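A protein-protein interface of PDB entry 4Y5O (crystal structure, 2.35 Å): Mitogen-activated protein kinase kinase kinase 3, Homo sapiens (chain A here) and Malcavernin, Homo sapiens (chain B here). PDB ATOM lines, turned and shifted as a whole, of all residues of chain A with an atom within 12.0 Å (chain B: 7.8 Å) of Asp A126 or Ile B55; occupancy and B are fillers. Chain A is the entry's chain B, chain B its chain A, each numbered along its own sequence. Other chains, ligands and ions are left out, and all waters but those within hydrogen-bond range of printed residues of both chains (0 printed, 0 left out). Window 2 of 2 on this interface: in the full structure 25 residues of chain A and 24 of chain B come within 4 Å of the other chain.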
ATOM      1  N   HIS A  53       5.475  38.425  26.251  1.00  0.00           N
ATOM      2  CA  HIS A  53       5.326  37.691  24.995  1.00  0.00           C
ATOM      3  C   HIS A  53       6.578  37.822  24.125  1.00  0.00           C
ATOM      4  O   HIS A  53       6.845  38.887  23.569  1.00  0.00           O
ATOM      5  CB  HIS A  53       4.096  38.181  24.225  1.00  0.00           C
ATOM      6  CG  HIS A  53       3.866  37.452  22.941  1.00  0.00           C
ATOM      7  ND1 HIS A  53       3.557  36.109  22.894  1.00  0.00           N
ATOM      8  CD2 HIS A  53       3.921  37.873  21.656  1.00  0.00           C
ATOM      9  CE1 HIS A  53       3.421  35.736  21.635  1.00  0.00           C
ATOM     10  NE2 HIS A  53       3.639  36.787  20.864  1.00  0.00           N
ATOM     11  N   ASN A  54       7.334  36.732  24.011  1.00  0.00           N
ATOM     12  CA  ASN A  54       8.642  36.731  23.347  1.00  0.00           C
ATOM     13  C   ASN A  54       9.578  37.850  23.791  1.00  0.00           C
ATOM     14  O   ASN A  54      10.236  38.476  22.959  1.00  0.00           O
ATOM     15  CB  ASN A  54       8.499  36.743  21.822  1.00  0.00           C
ATOM     16  CG  ASN A  54       7.721  35.551  21.299  1.00  0.00           C
ATOM     17  OD1 ASN A  54       7.717  34.480  21.905  1.00  0.00           O
ATOM     18  ND2 ASN A  54       7.056  35.733  20.164  1.00  0.00           N
ATOM     19  N   GLY A  80      -2.592  40.662  18.485  1.00  0.00           N
ATOM     20  CA  GLY A  80      -3.011  40.207  17.171  1.00  0.00           C
ATOM     21  C   GLY A  80      -3.166  38.715  16.943  1.00  0.00           C
ATOM     22  O   GLY A  80      -3.296  38.270  15.800  1.00  0.00           O
ATOM     23  N   GLN A  81      -3.154  37.938  18.015  1.00  0.00           N
ATOM     24  CA  GLN A  81      -3.360  36.502  17.886  1.00  0.00           C
ATOM     25  C   GLN A  81      -3.896  35.917  19.187  1.00  0.00           C
ATOM     26  O   GLN A  81      -3.667  36.468  20.251  1.00  0.00           O
ATOM     27  CB  GLN A  81      -2.058  35.812  17.489  1.00  0.00           C
ATOM     28  CG  GLN A  81      -0.915  36.072  18.442  1.00  0.00           C
ATOM     29  CD  GLN A  81       0.322  35.273  18.099  1.00  0.00           C
ATOM     30  OE1 GLN A  81       0.242  34.082  17.747  1.00  0.00           O
ATOM     31  NE2 GLN A  81       1.483  35.921  18.198  1.00  0.00           N
ATOM     32  N   PRO A  82      -4.634  34.804  19.104  1.00  0.00           N
ATOM     33  CA  PRO A  82      -5.095  34.177  20.350  1.00  0.00           C
ATOM     34  C   PRO A  82      -3.934  33.626  21.184  1.00  0.00           C
ATOM     35  O   PRO A  82      -3.176  32.772  20.714  1.00  0.00           O
ATOM     36  CB  PRO A  82      -5.982  33.031  19.853  1.00  0.00           C
ATOM     37  CG  PRO A  82      -5.496  32.746  18.458  1.00  0.00           C
ATOM     38  CD  PRO A  82      -5.123  34.095  17.911  1.00  0.00           C
ATOM     39  N   LEU A  83      -3.812  34.119  22.414  1.00  0.00           N
ATOM     40  CA  LEU A  83      -2.741  33.711  23.320  1.00  0.00           C
ATOM     41  C   LEU A  83      -3.281  33.164  24.657  1.00  0.00           C
ATOM     42  O   LEU A  83      -4.307  33.633  25.155  1.00  0.00           O
ATOM     43  CB  LEU A  83      -1.814  34.896  23.550  1.00  0.00           C
ATOM     44  CG  LEU A  83      -1.071  35.347  22.290  1.00  0.00           C
ATOM     45  CD1 LEU A  83      -0.222  36.600  22.537  1.00  0.00           C
ATOM     46  CD2 LEU A  83      -0.205  34.183  21.814  1.00  0.00           C
ATOM     47  N   ASP A  84      -2.607  32.166  25.226  1.00  0.00           N
ATOM     48  CA  ASP A  84      -2.977  31.637  26.545  1.00  0.00           C
ATOM     49  C   ASP A  84      -2.373  32.478  27.645  1.00  0.00           C
ATOM     50  O   ASP A  84      -1.237  32.944  27.516  1.00  0.00           O
ATOM     51  CB  ASP A  84      -2.508  30.190  26.707  1.00  0.00           C
ATOM     52  CG  ASP A  84      -3.440  29.204  26.045  1.00  0.00           C
ATOM     53  OD1 ASP A  84      -4.657  29.496  25.982  1.00  0.00           O
ATOM     54  OD2 ASP A  84      -2.953  28.144  25.589  1.00  0.00           O
ATOM     55  N   LEU A  85      -3.116  32.671  28.730  1.00  0.00           N
ATOM     56  CA  LEU A  85      -2.602  33.500  29.815  1.00  0.00           C
ATOM     57  C   LEU A  85      -2.033  32.615  30.915  1.00  0.00           C
ATOM     58  O   LEU A  85      -2.777  31.909  31.599  1.00  0.00           O
ATOM     59  CB  LEU A  85      -3.697  34.397  30.382  1.00  0.00           C
ATOM     60  CG  LEU A  85      -4.803  34.895  29.458  1.00  0.00           C
ATOM     61  CD1 LEU A  85      -5.876  35.609  30.260  1.00  0.00           C
ATOM     62  CD2 LEU A  85      -4.282  35.806  28.392  1.00  0.00           C
ATOM     63  N   HIS A  86      -0.717  32.636  31.088  1.00  0.00           N
ATOM     64  CA  HIS A  86      -0.118  31.841  32.145  1.00  0.00           C
ATOM     65  C   HIS A  86       0.214  32.713  33.354  1.00  0.00           C
ATOM     66  O   HIS A  86       1.187  33.474  33.334  1.00  0.00           O
ATOM     67  CB  HIS A  86       1.121  31.119  31.609  1.00  0.00           C
ATOM     68  CG  HIS A  86       0.804  30.080  30.573  1.00  0.00           C
ATOM     69  ND1 HIS A  86       0.568  28.760  30.892  1.00  0.00           N
ATOM     70  CD2 HIS A  86       0.680  30.167  29.228  1.00  0.00           C
ATOM     71  CE1 HIS A  86       0.317  28.080  29.789  1.00  0.00           C
ATOM     72  NE2 HIS A  86       0.381  28.908  28.765  1.00  0.00           N
ATOM     73  N   LEU A  95      -2.986  28.266  34.545  1.00  0.00           N
ATOM     74  CA  LEU A  95      -3.491  28.716  33.255  1.00  0.00           C
ATOM     75  C   LEU A  95      -4.844  29.362  33.511  1.00  0.00           C
ATOM     76  O   LEU A  95      -5.802  28.669  33.819  1.00  0.00           O
ATOM     77  CB  LEU A  95      -3.638  27.543  32.276  1.00  0.00           C
ATOM     78  CG  LEU A  95      -3.705  27.906  30.784  1.00  0.00           C
ATOM     79  CD1 LEU A  95      -3.391  26.726  29.903  1.00  0.00           C
ATOM     80  CD2 LEU A  95      -5.047  28.477  30.390  1.00  0.00           C
ATOM     81  N   LEU A 121       2.546  35.321  31.469  1.00  0.00           N
ATOM     82  CA  LEU A 121       3.324  34.857  30.328  1.00  0.00           C
ATOM     83  C   LEU A 121       2.390  34.468  29.190  1.00  0.00           C
ATOM     84  O   LEU A 121       1.494  33.655  29.375  1.00  0.00           O
ATOM     85  CB  LEU A 121       4.158  33.637  30.731  1.00  0.00           C
ATOM     86  CG  LEU A 121       4.937  32.904  29.641  1.00  0.00           C
ATOM     87  CD1 LEU A 121       5.988  33.813  29.031  1.00  0.00           C
ATOM     88  CD2 LEU A 121       5.584  31.638  30.200  1.00  0.00           C
ATOM     89  N   LEU A 122       2.597  35.031  28.007  1.00  0.00           N
ATOM     90  CA  LEU A 122       1.717  34.697  26.895  1.00  0.00           C
ATOM     91  C   LEU A 122       2.323  33.623  26.003  1.00  0.00           C
ATOM     92  O   LEU A 122       3.408  33.797  25.491  1.00  0.00           O
ATOM     93  CB  LEU A 122       1.363  35.954  26.090  1.00  0.00           C
ATOM     94  CG  LEU A 122       0.683  37.048  26.919  1.00  0.00           C
ATOM     95  CD1 LEU A 122       0.406  38.286  26.102  1.00  0.00           C
ATOM     96  CD2 LEU A 122      -0.598  36.533  27.543  1.00  0.00           C
ATOM     97  N   LEU A 123       1.620  32.506  25.836  1.00  0.00           N
ATOM     98  CA  LEU A 123       2.069  31.455  24.928  1.00  0.00           C
ATOM     99  C   LEU A 123       0.948  31.097  23.951  1.00  0.00           C
ATOM    100  O   LEU A 123      -0.222  31.315  24.240  1.00  0.00           O
ATOM    101  CB  LEU A 123       2.534  30.219  25.706  1.00  0.00           C
ATOM    102  CG  LEU A 123       3.688  30.433  26.690  1.00  0.00           C
ATOM    103  CD1 LEU A 123       3.959  29.180  27.505  1.00  0.00           C
ATOM    104  CD2 LEU A 123       4.951  30.871  25.968  1.00  0.00           C
ATOM    105  N   SER A 124       1.308  30.567  22.787  1.00  0.00           N
ATOM    106  CA  SER A 124       0.306  30.147  21.819  1.00  0.00           C
ATOM    107  C   SER A 124      -0.125  28.722  22.126  1.00  0.00           C
ATOM    108  O   SER A 124       0.700  27.893  22.517  1.00  0.00           O
ATOM    109  CB  SER A 124       0.867  30.225  20.401  1.00  0.00           C
ATOM    110  OG  SER A 124       1.610  29.057  20.095  1.00  0.00           O
ATOM    111  N   GLN A 125      -1.411  28.433  21.953  1.00  0.00           N
ATOM    112  CA  GLN A 125      -1.921  27.091  22.220  1.00  0.00           C
ATOM    113  C   GLN A 125      -1.378  26.079  21.213  1.00  0.00           C
ATOM    114  O   GLN A 125      -1.233  24.899  21.530  1.00  0.00           O
ATOM    115  CB  GLN A 125      -3.450  27.084  22.251  1.00  0.00           C
ATOM    116  CG  GLN A 125      -4.053  25.943  23.073  1.00  0.00           C
ATOM    117  CD  GLN A 125      -5.382  26.317  23.725  1.00  0.00           C
ATOM    118  OE1 GLN A 125      -5.511  27.376  24.339  1.00  0.00           O
ATOM    119  NE2 GLN A 125      -6.376  25.442  23.592  1.00  0.00           N
ATOM    120  N   ASP A 126      -1.063  26.547  20.008  1.00  0.00           N
ATOM    121  CA  ASP A 126      -0.449  25.699  18.989  1.00  0.00           C
ATOM    122  C   ASP A 126       0.740  26.392  18.341  1.00  0.00           C
ATOM    123  O   ASP A 126       0.763  27.616  18.217  1.00  0.00           O
ATOM    124  CB  ASP A 126      -1.466  25.310  17.914  1.00  0.00           C
ATOM    125  CG  ASP A 126      -2.174  24.007  18.224  1.00  0.00           C
ATOM    126  OD1 ASP A 126      -1.594  23.168  18.945  1.00  0.00           O
ATOM    127  OD2 ASP A 126      -3.310  23.821  17.739  1.00  0.00           O
ATOM    128  N   LEU B  40       5.443  27.025  34.395  1.00  0.00           N
ATOM    129  CA  LEU B  40       4.999  25.984  33.469  1.00  0.00           C
ATOM    130  C   LEU B  40       5.049  24.628  34.148  1.00  0.00           C
ATOM    131  O   LEU B  40       4.114  23.841  34.047  1.00  0.00           O
ATOM    132  CB  LEU B  40       5.855  25.953  32.207  1.00  0.00           C
ATOM    133  CG  LEU B  40       5.754  27.159  31.284  1.00  0.00           C
ATOM    134  CD1 LEU B  40       6.453  26.897  29.961  1.00  0.00           C
ATOM    135  CD2 LEU B  40       4.300  27.521  31.055  1.00  0.00           C
ATOM    136  N   SER B  49      -1.623  18.324  30.256  1.00  0.00           N
ATOM    137  CA  SER B  49      -1.130  17.284  29.359  1.00  0.00           C
ATOM    138  C   SER B  49       0.376  17.425  29.135  1.00  0.00           C
ATOM    139  O   SER B  49       0.987  18.411  29.539  1.00  0.00           O
ATOM    140  CB  SER B  49      -1.876  17.303  28.021  1.00  0.00           C
ATOM    141  OG  SER B  49      -1.099  17.913  27.005  1.00  0.00           O
ATOM    142  N   ILE B  50       0.967  16.417  28.507  1.00  0.00           N
ATOM    143  CA  ILE B  50       2.389  16.426  28.202  1.00  0.00           C
ATOM    144  C   ILE B  50       2.573  17.148  26.882  1.00  0.00           C
ATOM    145  O   ILE B  50       3.547  17.859  26.674  1.00  0.00           O
ATOM    146  CB  ILE B  50       2.938  14.980  28.109  1.00  0.00           C
ATOM    147  CG1 ILE B  50       4.393  14.965  27.629  1.00  0.00           C
ATOM    148  CG2 ILE B  50       2.056  14.131  27.195  1.00  0.00           C
ATOM    149  CD1 ILE B  50       5.379  15.480  28.644  1.00  0.00           C
ATOM    150  N   HIS B  51       1.614  16.957  25.988  1.00  0.00           N
ATOM    151  CA  HIS B  51       1.659  17.587  24.684  1.00  0.00           C
ATOM    152  C   HIS B  51       1.621  19.102  24.870  1.00  0.00           C
ATOM    153  O   HIS B  51       2.425  19.836  24.290  1.00  0.00           O
ATOM    154  CB  HIS B  51       0.484  17.097  23.842  1.00  0.00           C
ATOM    155  CG  HIS B  51       0.349  17.799  22.531  1.00  0.00           C
ATOM    156  ND1 HIS B  51       1.368  17.852  21.607  1.00  0.00           N
ATOM    157  CD2 HIS B  51      -0.688  18.488  21.992  1.00  0.00           C
ATOM    158  CE1 HIS B  51       0.966  18.539  20.552  1.00  0.00           C
ATOM    159  NE2 HIS B  51      -0.277  18.937  20.761  1.00  0.00           N
ATOM    160  N   GLU B  52       0.686  19.549  25.704  1.00  0.00           N
ATOM    161  CA  GLU B  52       0.591  20.939  26.123  1.00  0.00           C
ATOM    162  C   GLU B  52       1.926  21.455  26.644  1.00  0.00           C
ATOM    163  O   GLU B  52       2.464  22.449  26.147  1.00  0.00           O
ATOM    164  CB  GLU B  52      -0.463  21.055  27.226  1.00  0.00           C
ATOM    165  CG  GLU B  52      -0.656  22.447  27.773  1.00  0.00           C
ATOM    166  CD  GLU B  52      -1.305  23.369  26.766  1.00  0.00           C
ATOM    167  OE1 GLU B  52      -2.068  22.862  25.915  1.00  0.00           O
ATOM    168  OE2 GLU B  52      -1.046  24.593  26.821  1.00  0.00           O
ATOM    169  N   PHE B  53       2.452  20.766  27.651  1.00  0.00           N
ATOM    170  CA  PHE B  53       3.675  21.175  28.319  1.00  0.00           C
ATOM    171  C   PHE B  53       4.794  21.383  27.302  1.00  0.00           C
ATOM    172  O   PHE B  53       5.428  22.441  27.269  1.00  0.00           O
ATOM    173  CB  PHE B  53       4.070  20.120  29.354  1.00  0.00           C
ATOM    174  CG  PHE B  53       5.117  20.585  30.330  1.00  0.00           C
ATOM    175  CD1 PHE B  53       5.077  21.876  30.861  1.00  0.00           C
ATOM    176  CD2 PHE B  53       6.133  19.730  30.729  1.00  0.00           C
ATOM    177  CE1 PHE B  53       6.039  22.302  31.764  1.00  0.00           C
ATOM    178  CE2 PHE B  53       7.100  20.149  31.633  1.00  0.00           C
ATOM    179  CZ  PHE B  53       7.057  21.431  32.149  1.00  0.00           C
ATOM    180  N   CYS B  54       4.995  20.383  26.452  1.00  0.00           N
ATOM    181  CA  CYS B  54       6.021  20.420  25.411  1.00  0.00           C
ATOM    182  C   CYS B  54       5.869  21.594  24.449  1.00  0.00           C
ATOM    183  O   CYS B  54       6.849  22.251  24.097  1.00  0.00           O
ATOM    184  CB  CYS B  54       6.015  19.107  24.626  1.00  0.00           C
ATOM    185  SG  CYS B  54       6.490  17.674  25.607  1.00  0.00           S
ATOM    186  N   ILE B  55       4.641  21.846  24.016  1.00  0.00           N
ATOM    187  CA  ILE B  55       4.364  23.002  23.177  1.00  0.00           C
ATOM    188  C   ILE B  55       4.823  24.288  23.862  1.00  0.00           C
ATOM    189  O   ILE B  55       5.467  25.127  23.247  1.00  0.00           O
ATOM    190  CB  ILE B  55       2.872  23.100  22.849  1.00  0.00           C
ATOM    191  CG1 ILE B  55       2.452  21.954  21.941  1.00  0.00           C
ATOM    192  CG2 ILE B  55       2.561  24.425  22.175  1.00  0.00           C
ATOM    193  CD1 ILE B  55       0.961  21.947  21.608  1.00  0.00           C
ATOM    194  N   ASN B  56       4.507  24.420  25.144  1.00  0.00           N
ATOM    195  CA  ASN B  56       4.912  25.603  25.912  1.00  0.00           C
ATOM    196  C   ASN B  56       6.425  25.726  26.036  1.00  0.00           C
ATOM    197  O   ASN B  56       6.980  26.813  25.943  1.00  0.00           O
ATOM    198  CB  ASN B  56       4.265  25.589  27.301  1.00  0.00           C
ATOM    199  CG  ASN B  56       2.752  25.679  27.234  1.00  0.00           C
ATOM    200  OD1 ASN B  56       2.201  26.137  26.241  1.00  0.00           O
ATOM    201  ND2 ASN B  56       2.074  25.240  28.290  1.00  0.00           N
ATOM    202  N   LEU B  57       7.088  24.599  26.248  1.00  0.00           N
ATOM    203  CA  LEU B  57       8.537  24.585  26.359  1.00  0.00           C
ATOM    204  C   LEU B  57       9.183  25.012  25.047  1.00  0.00           C
ATOM    205  O   LEU B  57      10.106  25.818  25.034  1.00  0.00           O
ATOM    206  CB  LEU B  57       9.034  23.194  26.771  1.00  0.00           C
ATOM    207  CG  LEU B  57       9.249  22.906  28.263  1.00  0.00           C
ATOM    208  CD1 LEU B  57       9.434  24.181  29.050  1.00  0.00           C
ATOM    209  CD2 LEU B  57       8.116  22.097  28.859  1.00  0.00           C
ATOM    210  N   ARG B  58       8.673  24.476  23.946  1.00  0.00           N
ATOM    211  CA  ARG B  58       9.241  24.730  22.627  1.00  0.00           C
ATOM    212  C   ARG B  58       9.160  26.199  22.233  1.00  0.00           C
ATOM    213  O   ARG B  58       9.956  26.675  21.424  1.00  0.00           O
ATOM    214  CB  ARG B  58       8.528  23.873  21.579  1.00  0.00           C
ATOM    215  N   GLN B  59       8.193  26.911  22.801  1.00  0.00           N
ATOM    216  CA  GLN B  59       7.998  28.315  22.471  1.00  0.00           C
ATOM    217  C   GLN B  59       8.892  29.172  23.343  1.00  0.00           C
ATOM    218  O   GLN B  59       9.101  30.353  23.070  1.00  0.00           O
ATOM    219  CB  GLN B  59       6.548  28.739  22.720  1.00  0.00           C
ATOM    220  CG  GLN B  59       5.474  27.955  21.993  1.00  0.00           C
ATOM    221  CD  GLN B  59       4.080  28.445  22.338  1.00  0.00           C
ATOM    222  OE1 GLN B  59       3.877  29.633  22.602  1.00  0.00           O
ATOM    223  NE2 GLN B  59       3.115  27.538  22.338  1.00  0.00           N
ATOM    224  N   LEU B  60       9.405  28.576  24.411  1.00  0.00           N
ATOM    225  CA  LEU B  60      10.099  29.349  25.424  1.00  0.00           C
ATOM    226  C   LEU B  60      11.589  29.065  25.426  1.00  0.00           C
ATOM    227  O   LEU B  60      12.403  29.927  25.772  1.00  0.00           O
ATOM    228  CB  LEU B  60       9.510  29.042  26.791  1.00  0.00           C
ATOM    229  CG  LEU B  60       9.548  30.207  27.757  1.00  0.00           C
ATOM    230  CD1 LEU B  60       9.194  31.457  27.001  1.00  0.00           C
ATOM    231  CD2 LEU B  60       8.575  29.977  28.880  1.00  0.00           C
ATOM    232  N   TYR B  61      11.935  27.850  25.021  1.00  0.00           N
ATOM    233  CA  TYR B  61      13.308  27.377  25.091  1.00  0.00           C
ATOM    234  C   TYR B  61      13.807  26.800  23.761  1.00  0.00           C
ATOM    235  O   TYR B  61      13.459  25.680  23.384  1.00  0.00           O
ATOM    236  CB  TYR B  61      13.425  26.354  26.220  1.00  0.00           C
ATOM    237  CG  TYR B  61      13.003  26.939  27.536  1.00  0.00           C
ATOM    238  CD1 TYR B  61      13.657  28.043  28.052  1.00  0.00           C
ATOM    239  CD2 TYR B  61      11.941  26.409  28.254  1.00  0.00           C
ATOM    240  CE1 TYR B  61      13.279  28.601  29.244  1.00  0.00           C
ATOM    241  CE2 TYR B  61      11.560  26.956  29.458  1.00  0.00           C
ATOM    242  CZ  TYR B  61      12.233  28.057  29.949  1.00  0.00           C
ATOM    243  OH  TYR B  61      11.867  28.625  31.145  1.00  0.00           O
ATOM    244  N   PHE B  87       9.774  14.443  21.357  1.00  0.00           N
ATOM    245  CA  PHE B  87       9.709  15.908  21.435  1.00  0.00           C
ATOM    246  C   PHE B  87      11.084  16.567  21.296  1.00  0.00           C
ATOM    247  O   PHE B  87      11.186  17.739  20.926  1.00  0.00           O
ATOM    248  CB  PHE B  87       9.002  16.338  22.737  1.00  0.00           C
ATOM    249  CG  PHE B  87       9.103  17.816  23.047  1.00  0.00           C
ATOM    250  CD1 PHE B  87       8.575  18.768  22.184  1.00  0.00           C
ATOM    251  CD2 PHE B  87       9.705  18.247  24.220  1.00  0.00           C
ATOM    252  CE1 PHE B  87       8.669  20.120  22.476  1.00  0.00           C
ATOM    253  CE2 PHE B  87       9.802  19.595  24.518  1.00  0.00           C
ATOM    254  CZ  PHE B  87       9.286  20.529  23.645  1.00  0.00           C
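NE2 of Gln B59 is in hydrogen-bond range of O of Ser A124 (2.4 Å).
Among the printed residues, 10 pairs touch across the chains.
Among the printed residues, no Asp or Glu carboxylate lies within 4 Å of a Lys or Arg side-chain nitrogen of the other chain.
Leu B40 touches His A86.
His A86 touches Asn B56 (CE1 to ND2, 3.7 Å).
Leu A121 touches Leu B60 (CD2 to CD2, 3.7 Å).
CD1 of Leu A123 touches CD2 of Leu B40, 3.9 Å away.
CD1 of Leu A123 touches CB of Asn B56 (3.6 Å).
Gln B59 touches Leu A123 (OE1 to CB, 3.4 Å).
CG2 of Ile B55 touches O of Ser A124, at 3.95 Å.
Ile B55 touches Gln A125 (CD1 to O, 3.7 Å).
OD1 of Asp A126 touches CD1 of Ile B55 (3.9 Å).
NE2 of Gln B59 sits close to O of Ile B55, 3.5 Å away.
The backbone carbonyl oxygen of Leu A123 lies within hydrogen-bond range of the backbone NH of Asp A84, at 2.7 Å.
The side-chain carboxylate of Asp A84 lies close to the side-chain amide oxygen of Gln A125.
The backbone NH (N) of Leu A121 is in hydrogen-bond range of the backbone carbonyl oxygen (O) of His A86 (3.0 Å).
The side-chain hydroxyl (OG) of Ser A124 sits at hydrogen-bond distance from the backbone carbonyl oxygen (O) of Asp A126, 2.5 Å away.
Asp A126 touches one residue of chain B.
Ile B55 touches just these residues of chain A: Ser A124, Gln A125 and Asp A126.
No residue of chain A comes within 4 Å of His B51.
No residue of chain A comes within 4 Å of Cys B54.
Of the printed residues of chain A, Asn B56 touches His A86 (3.7 Å) and Leu A123 (3.6 Å).
Gln B59 touches just these residues of chain A: Leu A123 (3.4 Å) and Ser A124 (2.4 Å).
Of the printed residues of chain B, Ser A124 touches Ile B55 and Gln B59.
Printed residues of chain B within 4 Å of Leu A121: Leu B60.
Printed residues of chain B within 4 Å of His A86: Leu B40 (3.9 Å) and Asn B56 (3.7 Å).
Printed residues of chain A within 4 Å of Leu B60: Leu A121 (3.7 Å).
The nearest printed residue of chain B that does not touch Gln A125 is Gln B59 (4.6 Å).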
